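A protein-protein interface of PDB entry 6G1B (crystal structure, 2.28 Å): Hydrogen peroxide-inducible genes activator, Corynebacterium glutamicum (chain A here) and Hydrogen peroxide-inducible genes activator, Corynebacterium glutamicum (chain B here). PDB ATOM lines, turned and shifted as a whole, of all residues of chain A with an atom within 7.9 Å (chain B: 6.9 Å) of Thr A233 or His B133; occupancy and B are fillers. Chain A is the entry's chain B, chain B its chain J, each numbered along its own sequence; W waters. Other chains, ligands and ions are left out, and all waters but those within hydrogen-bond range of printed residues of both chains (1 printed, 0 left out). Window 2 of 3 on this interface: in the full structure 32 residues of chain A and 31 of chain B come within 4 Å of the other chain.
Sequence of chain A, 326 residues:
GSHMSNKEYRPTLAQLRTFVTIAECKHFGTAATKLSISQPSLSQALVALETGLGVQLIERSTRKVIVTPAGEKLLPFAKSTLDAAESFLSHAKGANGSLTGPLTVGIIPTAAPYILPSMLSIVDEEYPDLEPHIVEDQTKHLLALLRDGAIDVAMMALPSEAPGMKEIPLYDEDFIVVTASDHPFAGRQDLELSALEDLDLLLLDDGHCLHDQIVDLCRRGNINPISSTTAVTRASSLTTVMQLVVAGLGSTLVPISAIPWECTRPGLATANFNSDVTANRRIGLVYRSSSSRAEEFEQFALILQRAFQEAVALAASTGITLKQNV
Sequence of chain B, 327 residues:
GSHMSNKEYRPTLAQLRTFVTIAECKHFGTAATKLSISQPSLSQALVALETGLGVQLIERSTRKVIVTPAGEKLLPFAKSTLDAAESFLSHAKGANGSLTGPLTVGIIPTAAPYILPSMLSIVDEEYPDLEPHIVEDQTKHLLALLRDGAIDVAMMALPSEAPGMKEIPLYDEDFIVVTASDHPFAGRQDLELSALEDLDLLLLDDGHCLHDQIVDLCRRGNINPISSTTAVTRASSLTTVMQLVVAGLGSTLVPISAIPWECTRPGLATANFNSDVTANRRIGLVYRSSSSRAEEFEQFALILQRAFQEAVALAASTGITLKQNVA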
ATOM      1  N   LEU A 201      -4.789 -28.226   3.371  1.00  0.00           N
ATOM      2  CA  LEU A 201      -3.766 -27.865   4.352  1.00  0.00           C
ATOM      3  C   LEU A 201      -3.642 -26.345   4.509  1.00  0.00           C
ATOM      4  O   LEU A 201      -3.577 -25.609   3.527  1.00  0.00           O
ATOM      5  CB  LEU A 201      -2.386 -28.416   3.965  1.00  0.00           C
ATOM      6  CG  LEU A 201      -2.008 -29.860   4.232  1.00  0.00           C
ATOM      7  CD1 LEU A 201      -0.516 -29.976   3.987  1.00  0.00           C
ATOM      8  CD2 LEU A 201      -2.264 -30.367   5.642  1.00  0.00           C
ATOM      9  N   LEU A 202      -3.668 -25.892   5.752  1.00  0.00           N
ATOM     10  CA  LEU A 202      -3.343 -24.534   6.102  1.00  0.00           C
ATOM     11  C   LEU A 202      -2.003 -24.649   6.827  1.00  0.00           C
ATOM     12  O   LEU A 202      -1.870 -25.299   7.859  1.00  0.00           O
ATOM     13  CB  LEU A 202      -4.384 -23.980   7.042  1.00  0.00           C
ATOM     14  CG  LEU A 202      -5.853 -24.210   6.741  1.00  0.00           C
ATOM     15  CD1 LEU A 202      -6.568 -24.834   7.954  1.00  0.00           C
ATOM     16  CD2 LEU A 202      -6.483 -22.889   6.364  1.00  0.00           C
ATOM     17  N   LEU A 203      -1.002 -24.050   6.207  1.00  0.00           N
ATOM     18  CA  LEU A 203       0.376 -24.218   6.579  1.00  0.00           C
ATOM     19  C   LEU A 203       0.885 -22.921   7.149  1.00  0.00           C
ATOM     20  O   LEU A 203       0.465 -21.855   6.737  1.00  0.00           O
ATOM     21  CB  LEU A 203       1.191 -24.584   5.350  1.00  0.00           C
ATOM     22  CG  LEU A 203       0.824 -25.937   4.705  1.00  0.00           C
ATOM     23  CD1 LEU A 203       1.399 -26.050   3.299  1.00  0.00           C
ATOM     24  CD2 LEU A 203       1.249 -27.107   5.576  1.00  0.00           C
ATOM     25  N   ASN A 224       6.248 -20.116  -2.704  1.00  0.00           N
ATOM     26  CA  ASN A 224       5.709 -21.267  -1.989  1.00  0.00           C
ATOM     27  C   ASN A 224       4.990 -22.130  -3.008  1.00  0.00           C
ATOM     28  O   ASN A 224       4.037 -21.667  -3.610  1.00  0.00           O
ATOM     29  CB  ASN A 224       4.760 -20.791  -0.877  1.00  0.00           C
ATOM     30  CG  ASN A 224       4.130 -21.935  -0.091  1.00  0.00           C
ATOM     31  OD1 ASN A 224       4.445 -23.111  -0.289  1.00  0.00           O
ATOM     32  ND2 ASN A 224       3.215 -21.587   0.802  1.00  0.00           N
ATOM     33  N   SER A 227      -0.081 -24.121  -2.490  1.00  0.00           N
ATOM     34  CA  SER A 227      -1.058 -23.049  -2.306  1.00  0.00           C
ATOM     35  C   SER A 227      -2.219 -23.517  -1.436  1.00  0.00           C
ATOM     36  O   SER A 227      -2.482 -24.722  -1.308  1.00  0.00           O
ATOM     37  CB  SER A 227      -1.620 -22.606  -3.652  1.00  0.00           C
ATOM     38  OG  SER A 227      -0.615 -21.995  -4.409  1.00  0.00           O
ATOM     39  N   SER A 228      -2.917 -22.541  -0.868  1.00  0.00           N
ATOM     40  CA  SER A 228      -4.113 -22.797  -0.086  1.00  0.00           C
ATOM     41  C   SER A 228      -5.326 -22.438  -0.908  1.00  0.00           C
ATOM     42  O   SER A 228      -5.317 -21.474  -1.669  1.00  0.00           O
ATOM     43  CB  SER A 228      -4.092 -22.005   1.215  1.00  0.00           C
ATOM     44  OG  SER A 228      -3.316 -22.692   2.192  1.00  0.00           O
ATOM     45  N   THR A 229      -6.372 -23.224  -0.702  1.00  0.00           N
ATOM     46  CA  THR A 229      -7.600 -23.178  -1.500  1.00  0.00           C
ATOM     47  C   THR A 229      -8.790 -22.806  -0.600  1.00  0.00           C
ATOM     48  O   THR A 229      -9.957 -23.091  -0.926  1.00  0.00           O
ATOM     49  CB  THR A 229      -7.845 -24.560  -2.141  1.00  0.00           C
ATOM     50  OG1 THR A 229      -9.099 -24.571  -2.845  1.00  0.00           O
ATOM     51  CG2 THR A 229      -7.815 -25.679  -1.078  1.00  0.00           C
ATOM     52  N   THR A 230      -8.470 -22.093   0.480  1.00  0.00           N
ATOM     53  CA  THR A 230      -9.361 -21.866   1.620  1.00  0.00           C
ATOM     54  C   THR A 230      -9.596 -20.370   1.804  1.00  0.00           C
ATOM     55  O   THR A 230      -8.901 -19.547   1.196  1.00  0.00           O
ATOM     56  CB  THR A 230      -8.774 -22.436   2.942  1.00  0.00           C
ATOM     57  OG1 THR A 230      -9.651 -22.114   4.027  1.00  0.00           O
ATOM     58  CG2 THR A 230      -7.375 -21.864   3.263  1.00  0.00           C
ATOM     59  N   ALA A 231     -10.584 -20.006   2.629  1.00  0.00           N
ATOM     60  CA  ALA A 231     -10.840 -18.599   2.966  1.00  0.00           C
ATOM     61  C   ALA A 231      -9.663 -17.925   3.680  1.00  0.00           C
ATOM     62  O   ALA A 231      -9.547 -16.713   3.650  1.00  0.00           O
ATOM     63  CB  ALA A 231     -12.104 -18.470   3.804  1.00  0.00           C
ATOM     64  N   VAL A 232      -8.832 -18.709   4.346  1.00  0.00           N
ATOM     65  CA  VAL A 232      -7.621 -18.230   5.017  1.00  0.00           C
ATOM     66  C   VAL A 232      -6.403 -18.253   4.098  1.00  0.00           C
ATOM     67  O   VAL A 232      -5.748 -19.273   3.934  1.00  0.00           O
ATOM     68  CB  VAL A 232      -7.320 -19.048   6.280  1.00  0.00           C
ATOM     69  CG1 VAL A 232      -6.097 -18.481   7.000  1.00  0.00           C
ATOM     70  CG2 VAL A 232      -8.553 -19.092   7.175  1.00  0.00           C
ATOM     71  N   THR A 233      -6.111 -17.091   3.512  1.00  0.00           N
ATOM     72  CA  THR A 233      -4.887 -16.855   2.767  1.00  0.00           C
ATOM     73  C   THR A 233      -3.624 -17.181   3.554  1.00  0.00           C
ATOM     74  O   THR A 233      -2.739 -17.843   3.052  1.00  0.00           O
ATOM     75  CB  THR A 233      -4.831 -15.399   2.312  1.00  0.00           C
ATOM     76  OG1 THR A 233      -6.007 -15.149   1.535  1.00  0.00           O
ATOM     77  CG2 THR A 233      -3.579 -15.104   1.445  1.00  0.00           C
ATOM     78  N   ARG A 234      -3.541 -16.702   4.787  1.00  0.00           N
ATOM     79  CA  ARG A 234      -2.294 -16.735   5.567  1.00  0.00           C
ATOM     80  C   ARG A 234      -2.611 -16.685   7.076  1.00  0.00           C
ATOM     81  O   ARG A 234      -3.261 -15.745   7.498  1.00  0.00           O
ATOM     82  CB  ARG A 234      -1.449 -15.513   5.162  1.00  0.00           C
ATOM     83  CG  ARG A 234       0.051 -15.708   5.188  1.00  0.00           C
ATOM     84  CD  ARG A 234       0.780 -14.369   5.068  1.00  0.00           C
ATOM     85  NE  ARG A 234       0.286 -13.515   3.967  1.00  0.00           N
ATOM     86  CZ  ARG A 234       0.332 -12.177   3.946  1.00  0.00           C
ATOM     87  NH1 ARG A 234       0.854 -11.489   4.966  1.00  0.00           N
ATOM     88  NH2 ARG A 234      -0.151 -11.511   2.890  1.00  0.00           N
ATOM     89  N   ALA A 235      -2.142 -17.658   7.848  1.00  0.00           N
ATOM     90  CA  ALA A 235      -2.275 -17.666   9.309  1.00  0.00           C
ATOM     91  C   ALA A 235      -0.879 -17.592   9.884  1.00  0.00           C
ATOM     92  O   ALA A 235       0.061 -18.157   9.324  1.00  0.00           O
ATOM     93  CB  ALA A 235      -2.968 -18.925   9.770  1.00  0.00           C
ATOM     94  N   GLY B 101     -18.522 -10.169  -3.520  1.00  0.00           N
ATOM     95  CA  GLY B 101     -17.185 -10.145  -4.055  1.00  0.00           C
ATOM     96  C   GLY B 101     -16.080 -10.284  -2.997  1.00  0.00           C
ATOM     97  O   GLY B 101     -16.350 -10.679  -1.855  1.00  0.00           O
ATOM     98  N   PRO B 102     -14.829  -9.997  -3.394  1.00  0.00           N
ATOM     99  CA  PRO B 102     -13.686 -10.211  -2.525  1.00  0.00           C
ATOM    100  C   PRO B 102     -13.664  -9.255  -1.340  1.00  0.00           C
ATOM    101  O   PRO B 102     -13.917  -8.067  -1.503  1.00  0.00           O
ATOM    102  CB  PRO B 102     -12.475  -9.929  -3.450  1.00  0.00           C
ATOM    103  CG  PRO B 102     -13.015  -9.804  -4.833  1.00  0.00           C
ATOM    104  CD  PRO B 102     -14.440  -9.425  -4.696  1.00  0.00           C
ATOM    105  N   LEU B 103     -13.380  -9.784  -0.165  1.00  0.00           N
ATOM    106  CA  LEU B 103     -13.093  -8.958   1.002  1.00  0.00           C
ATOM    107  C   LEU B 103     -11.895  -9.568   1.703  1.00  0.00           C
ATOM    108  O   LEU B 103     -11.989 -10.661   2.234  1.00  0.00           O
ATOM    109  CB  LEU B 103     -14.311  -8.878   1.933  1.00  0.00           C
ATOM    110  CG  LEU B 103     -14.118  -8.013   3.186  1.00  0.00           C
ATOM    111  CD1 LEU B 103     -13.826  -6.570   2.864  1.00  0.00           C
ATOM    112  CD2 LEU B 103     -15.345  -8.063   4.064  1.00  0.00           C
ATOM    113  N   THR B 104     -10.775  -8.865   1.681  1.00  0.00           N
ATOM    114  CA  THR B 104      -9.570  -9.330   2.335  1.00  0.00           C
ATOM    115  C   THR B 104      -9.409  -8.662   3.738  1.00  0.00           C
ATOM    116  O   THR B 104      -9.279  -7.439   3.851  1.00  0.00           O
ATOM    117  CB  THR B 104      -8.369  -9.123   1.429  1.00  0.00           C
ATOM    118  OG1 THR B 104      -8.624  -9.801   0.194  1.00  0.00           O
ATOM    119  CG2 THR B 104      -7.106  -9.680   2.054  1.00  0.00           C
ATOM    120  N   VAL B 105      -9.427  -9.493   4.782  1.00  0.00           N
ATOM    121  CA  VAL B 105      -9.464  -9.037   6.167  1.00  0.00           C
ATOM    122  C   VAL B 105      -8.187  -9.437   6.927  1.00  0.00           C
ATOM    123  O   VAL B 105      -7.864 -10.618   6.991  1.00  0.00           O
ATOM    124  CB  VAL B 105     -10.694  -9.632   6.913  1.00  0.00           C
ATOM    125  CG1 VAL B 105     -10.905  -8.957   8.255  1.00  0.00           C
ATOM    126  CG2 VAL B 105     -11.965  -9.456   6.077  1.00  0.00           C
ATOM    127  N   GLY B 106      -7.480  -8.450   7.489  1.00  0.00           N
ATOM    128  CA  GLY B 106      -6.417  -8.713   8.469  1.00  0.00           C
ATOM    129  C   GLY B 106      -6.998  -8.870   9.873  1.00  0.00           C
ATOM    130  O   GLY B 106      -7.883  -8.118  10.230  1.00  0.00           O
ATOM    131  N   LEU B 120     -16.703 -17.071   9.738  1.00  0.00           N
ATOM    132  CA  LEU B 120     -16.725 -17.781   8.465  1.00  0.00           C
ATOM    133  C   LEU B 120     -18.022 -18.559   8.234  1.00  0.00           C
ATOM    134  O   LEU B 120     -18.525 -18.619   7.122  1.00  0.00           O
ATOM    135  CB  LEU B 120     -15.513 -18.714   8.311  1.00  0.00           C
ATOM    136  CG  LEU B 120     -14.165 -18.031   8.156  1.00  0.00           C
ATOM    137  CD1 LEU B 120     -13.056 -19.071   8.178  1.00  0.00           C
ATOM    138  CD2 LEU B 120     -14.094 -17.221   6.856  1.00  0.00           C
ATOM    139  N   GLU B 131     -16.779 -13.200  -0.729  1.00  0.00           N
ATOM    140  CA  GLU B 131     -15.627 -14.044  -0.919  1.00  0.00           C
ATOM    141  C   GLU B 131     -14.556 -13.593   0.089  1.00  0.00           C
ATOM    142  O   GLU B 131     -13.747 -12.712  -0.204  1.00  0.00           O
ATOM    143  CB  GLU B 131     -15.151 -13.918  -2.374  1.00  0.00           C
ATOM    144  CG  GLU B 131     -16.148 -14.369  -3.428  1.00  0.00           C
ATOM    145  CD  GLU B 131     -15.618 -14.238  -4.870  1.00  0.00           C
ATOM    146  OE1 GLU B 131     -14.377 -14.083  -5.129  1.00  0.00           O
ATOM    147  OE2 GLU B 131     -16.459 -14.302  -5.781  1.00  0.00           O
ATOM    148  N   PRO B 132     -14.579 -14.157   1.301  1.00  0.00           N
ATOM    149  CA  PRO B 132     -13.674 -13.648   2.344  1.00  0.00           C
ATOM    150  C   PRO B 132     -12.260 -14.197   2.169  1.00  0.00           C
ATOM    151  O   PRO B 132     -12.104 -15.365   1.785  1.00  0.00           O
ATOM    152  CB  PRO B 132     -14.286 -14.181   3.643  1.00  0.00           C
ATOM    153  CG  PRO B 132     -14.971 -15.438   3.229  1.00  0.00           C
ATOM    154  CD  PRO B 132     -15.435 -15.249   1.793  1.00  0.00           C
ATOM    155  N   HIS B 133     -11.250 -13.356   2.405  1.00  0.00           N
ATOM    156  CA  HIS B 133      -9.856 -13.782   2.452  1.00  0.00           C
ATOM    157  C   HIS B 133      -9.240 -13.267   3.738  1.00  0.00           C
ATOM    158  O   HIS B 133      -9.243 -12.064   3.970  1.00  0.00           O
ATOM    159  CB  HIS B 133      -9.095 -13.258   1.234  1.00  0.00           C
ATOM    160  CG  HIS B 133      -9.654 -13.761  -0.053  1.00  0.00           C
ATOM    161  ND1 HIS B 133      -9.467 -15.057  -0.479  1.00  0.00           N
ATOM    162  CD2 HIS B 133     -10.460 -13.170  -0.970  1.00  0.00           C
ATOM    163  CE1 HIS B 133     -10.122 -15.241  -1.617  1.00  0.00           C
ATOM    164  NE2 HIS B 133     -10.744 -14.117  -1.931  1.00  0.00           N
ATOM    165  N   ILE B 134      -8.715 -14.163   4.567  1.00  0.00           N
ATOM    166  CA  ILE B 134      -8.231 -13.806   5.889  1.00  0.00           C
ATOM    167  C   ILE B 134      -6.722 -13.912   5.963  1.00  0.00           C
ATOM    168  O   ILE B 134      -6.145 -14.930   5.540  1.00  0.00           O
ATOM    169  CB  ILE B 134      -8.818 -14.729   6.990  1.00  0.00           C
ATOM    170  CG1 ILE B 134     -10.338 -14.858   6.872  1.00  0.00           C
ATOM    171  CG2 ILE B 134      -8.434 -14.225   8.366  1.00  0.00           C
ATOM    172  CD1 ILE B 134     -11.088 -13.558   7.059  1.00  0.00           C
ATOM    173  N   VAL B 135      -6.115 -12.856   6.495  1.00  0.00           N
ATOM    174  CA  VAL B 135      -4.714 -12.786   6.825  1.00  0.00           C
ATOM    175  C   VAL B 135      -4.635 -12.548   8.331  1.00  0.00           C
ATOM    176  O   VAL B 135      -5.153 -11.572   8.833  1.00  0.00           O
ATOM    177  CB  VAL B 135      -4.007 -11.635   6.055  1.00  0.00           C
ATOM    178  CG1 VAL B 135      -2.574 -11.456   6.513  1.00  0.00           C
ATOM    179  CG2 VAL B 135      -3.979 -11.938   4.569  1.00  0.00           C
ATOM    180  N   GLU B 136      -3.978 -13.444   9.048  1.00  0.00           N
ATOM    181  CA  GLU B 136      -3.752 -13.300  10.477  1.00  0.00           C
ATOM    182  C   GLU B 136      -2.293 -12.946  10.711  1.00  0.00           C
ATOM    183  O   GLU B 136      -1.413 -13.697  10.308  1.00  0.00           O
ATOM    184  CB  GLU B 136      -4.124 -14.587  11.199  1.00  0.00           C
ATOM    185  CG  GLU B 136      -3.979 -14.520  12.720  1.00  0.00           C
ATOM    186  CD  GLU B 136      -3.362 -15.746  13.346  1.00  0.00           C
ATOM    187  OE1 GLU B 136      -2.953 -16.694  12.688  1.00  0.00           O
ATOM    188  OE2 GLU B 136      -3.311 -15.804  14.558  1.00  0.00           O
ATOM    189  N   ILE B 151      -4.378  -5.774   2.065  1.00  0.00           N
ATOM    190  CA  ILE B 151      -5.684  -6.066   2.690  1.00  0.00           C
ATOM    191  C   ILE B 151      -6.609  -4.869   2.546  1.00  0.00           C
ATOM    192  O   ILE B 151      -6.150  -3.766   2.264  1.00  0.00           O
ATOM    193  CB  ILE B 151      -5.566  -6.514   4.165  1.00  0.00           C
ATOM    194  CG1 ILE B 151      -5.114  -5.359   5.073  1.00  0.00           C
ATOM    195  CG2 ILE B 151      -4.628  -7.712   4.279  1.00  0.00           C
ATOM    196  CD1 ILE B 151      -4.935  -5.774   6.514  1.00  0.00           C
ATOM    197  N   ASP B 152      -7.902  -5.095   2.743  1.00  0.00           N
ATOM    198  CA  ASP B 152      -8.924  -4.045   2.618  1.00  0.00           C
ATOM    199  C   ASP B 152      -9.242  -3.399   3.980  1.00  0.00           C
ATOM    200  O   ASP B 152      -9.564  -2.196   4.070  1.00  0.00           O
ATOM    201  CB  ASP B 152     -10.236  -4.641   2.038  1.00  0.00           C
ATOM    202  CG  ASP B 152      -9.988  -5.599   0.790  1.00  0.00           C
ATOM    203  OD1 ASP B 152      -8.876  -5.502   0.175  1.00  0.00           O
ATOM    204  OD2 ASP B 152     -10.870  -6.454   0.437  1.00  0.00           O
HETATM  205  O   HOH W   1      -7.969 -16.879   0.604  1.00  0.00           O
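Of the 13 printed residues of chain A, 5 touch a printed residue of chain B. Of the 15 printed residues of chain B, 6 touch a printed residue of chain A. Among the printed residues, 11 pairs touch across the chains. Among the printed residues, no Asp or Glu carboxylate lies within 4 Å of a Lys or Arg side-chain nitrogen of the other chain.
O of Pro B132 sits close to O of Ala A231, at 3.4 Å. N of Glu B136 sits at hydrogen-bond distance from O of Arg A234. The backbone carbonyl oxygen (O) of Ile B134 lies within hydrogen-bond range of the backbone NH (N) of Arg A234 (3.2 Å). N of Ile B134 sits at hydrogen-bond distance from O of Ala A231, at 2.8 Å. O of Ile B134 is in hydrogen-bond range of N of Thr A233 (3.0 Å).
N of Val B105 lies within hydrogen-bond range of O of His B133 (2.7 Å). O of Leu B103 is in hydrogen-bond range of N of His B133 (2.8 Å). O of Val B105 lies within hydrogen-bond range of N of Val B135 (2.9 Å).
Among the printed residues, pairs that only touch across the chains: Ala A231 with Leu B120, Ala A231 with His B133, Val A232 with Ile B134, Thr A233 with His B133, Arg A234 with Val B135 and Ala A235 with Glu B136.
Water W1 lies within hydrogen-bond range of ND1 of His B133 (2.6 Å), OG1 of Thr A233 (2.8 Å), O of Thr A230 (2.9 Å) and O of Ala A231 (3.4 Å).
Thr A233 touches two residues of chain B. Of chain A, only Ala A231 and Thr A233 come within 4 Å of His B133. Of the printed residues of chain A, Val B135 touches Arg A234. Of the printed residues of chain B, Arg A234 touches Ile B134, Val B135 and Glu B136. Printed residues of chain B within 4 Å of Ala A235: Glu B136 (3.6 Å). Of the printed residues of chain B, Ala A231 touches Leu B120, Pro B132, His B133 and Ile B134. Ser A227 touches none of the printed residues of chain B. The nearest residue of chain B that does not touch Thr A233 is Val B135 (4.2 Å). The nearest printed residue of chain A that does not touch His B133 is Thr A230 (4.8 Å).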
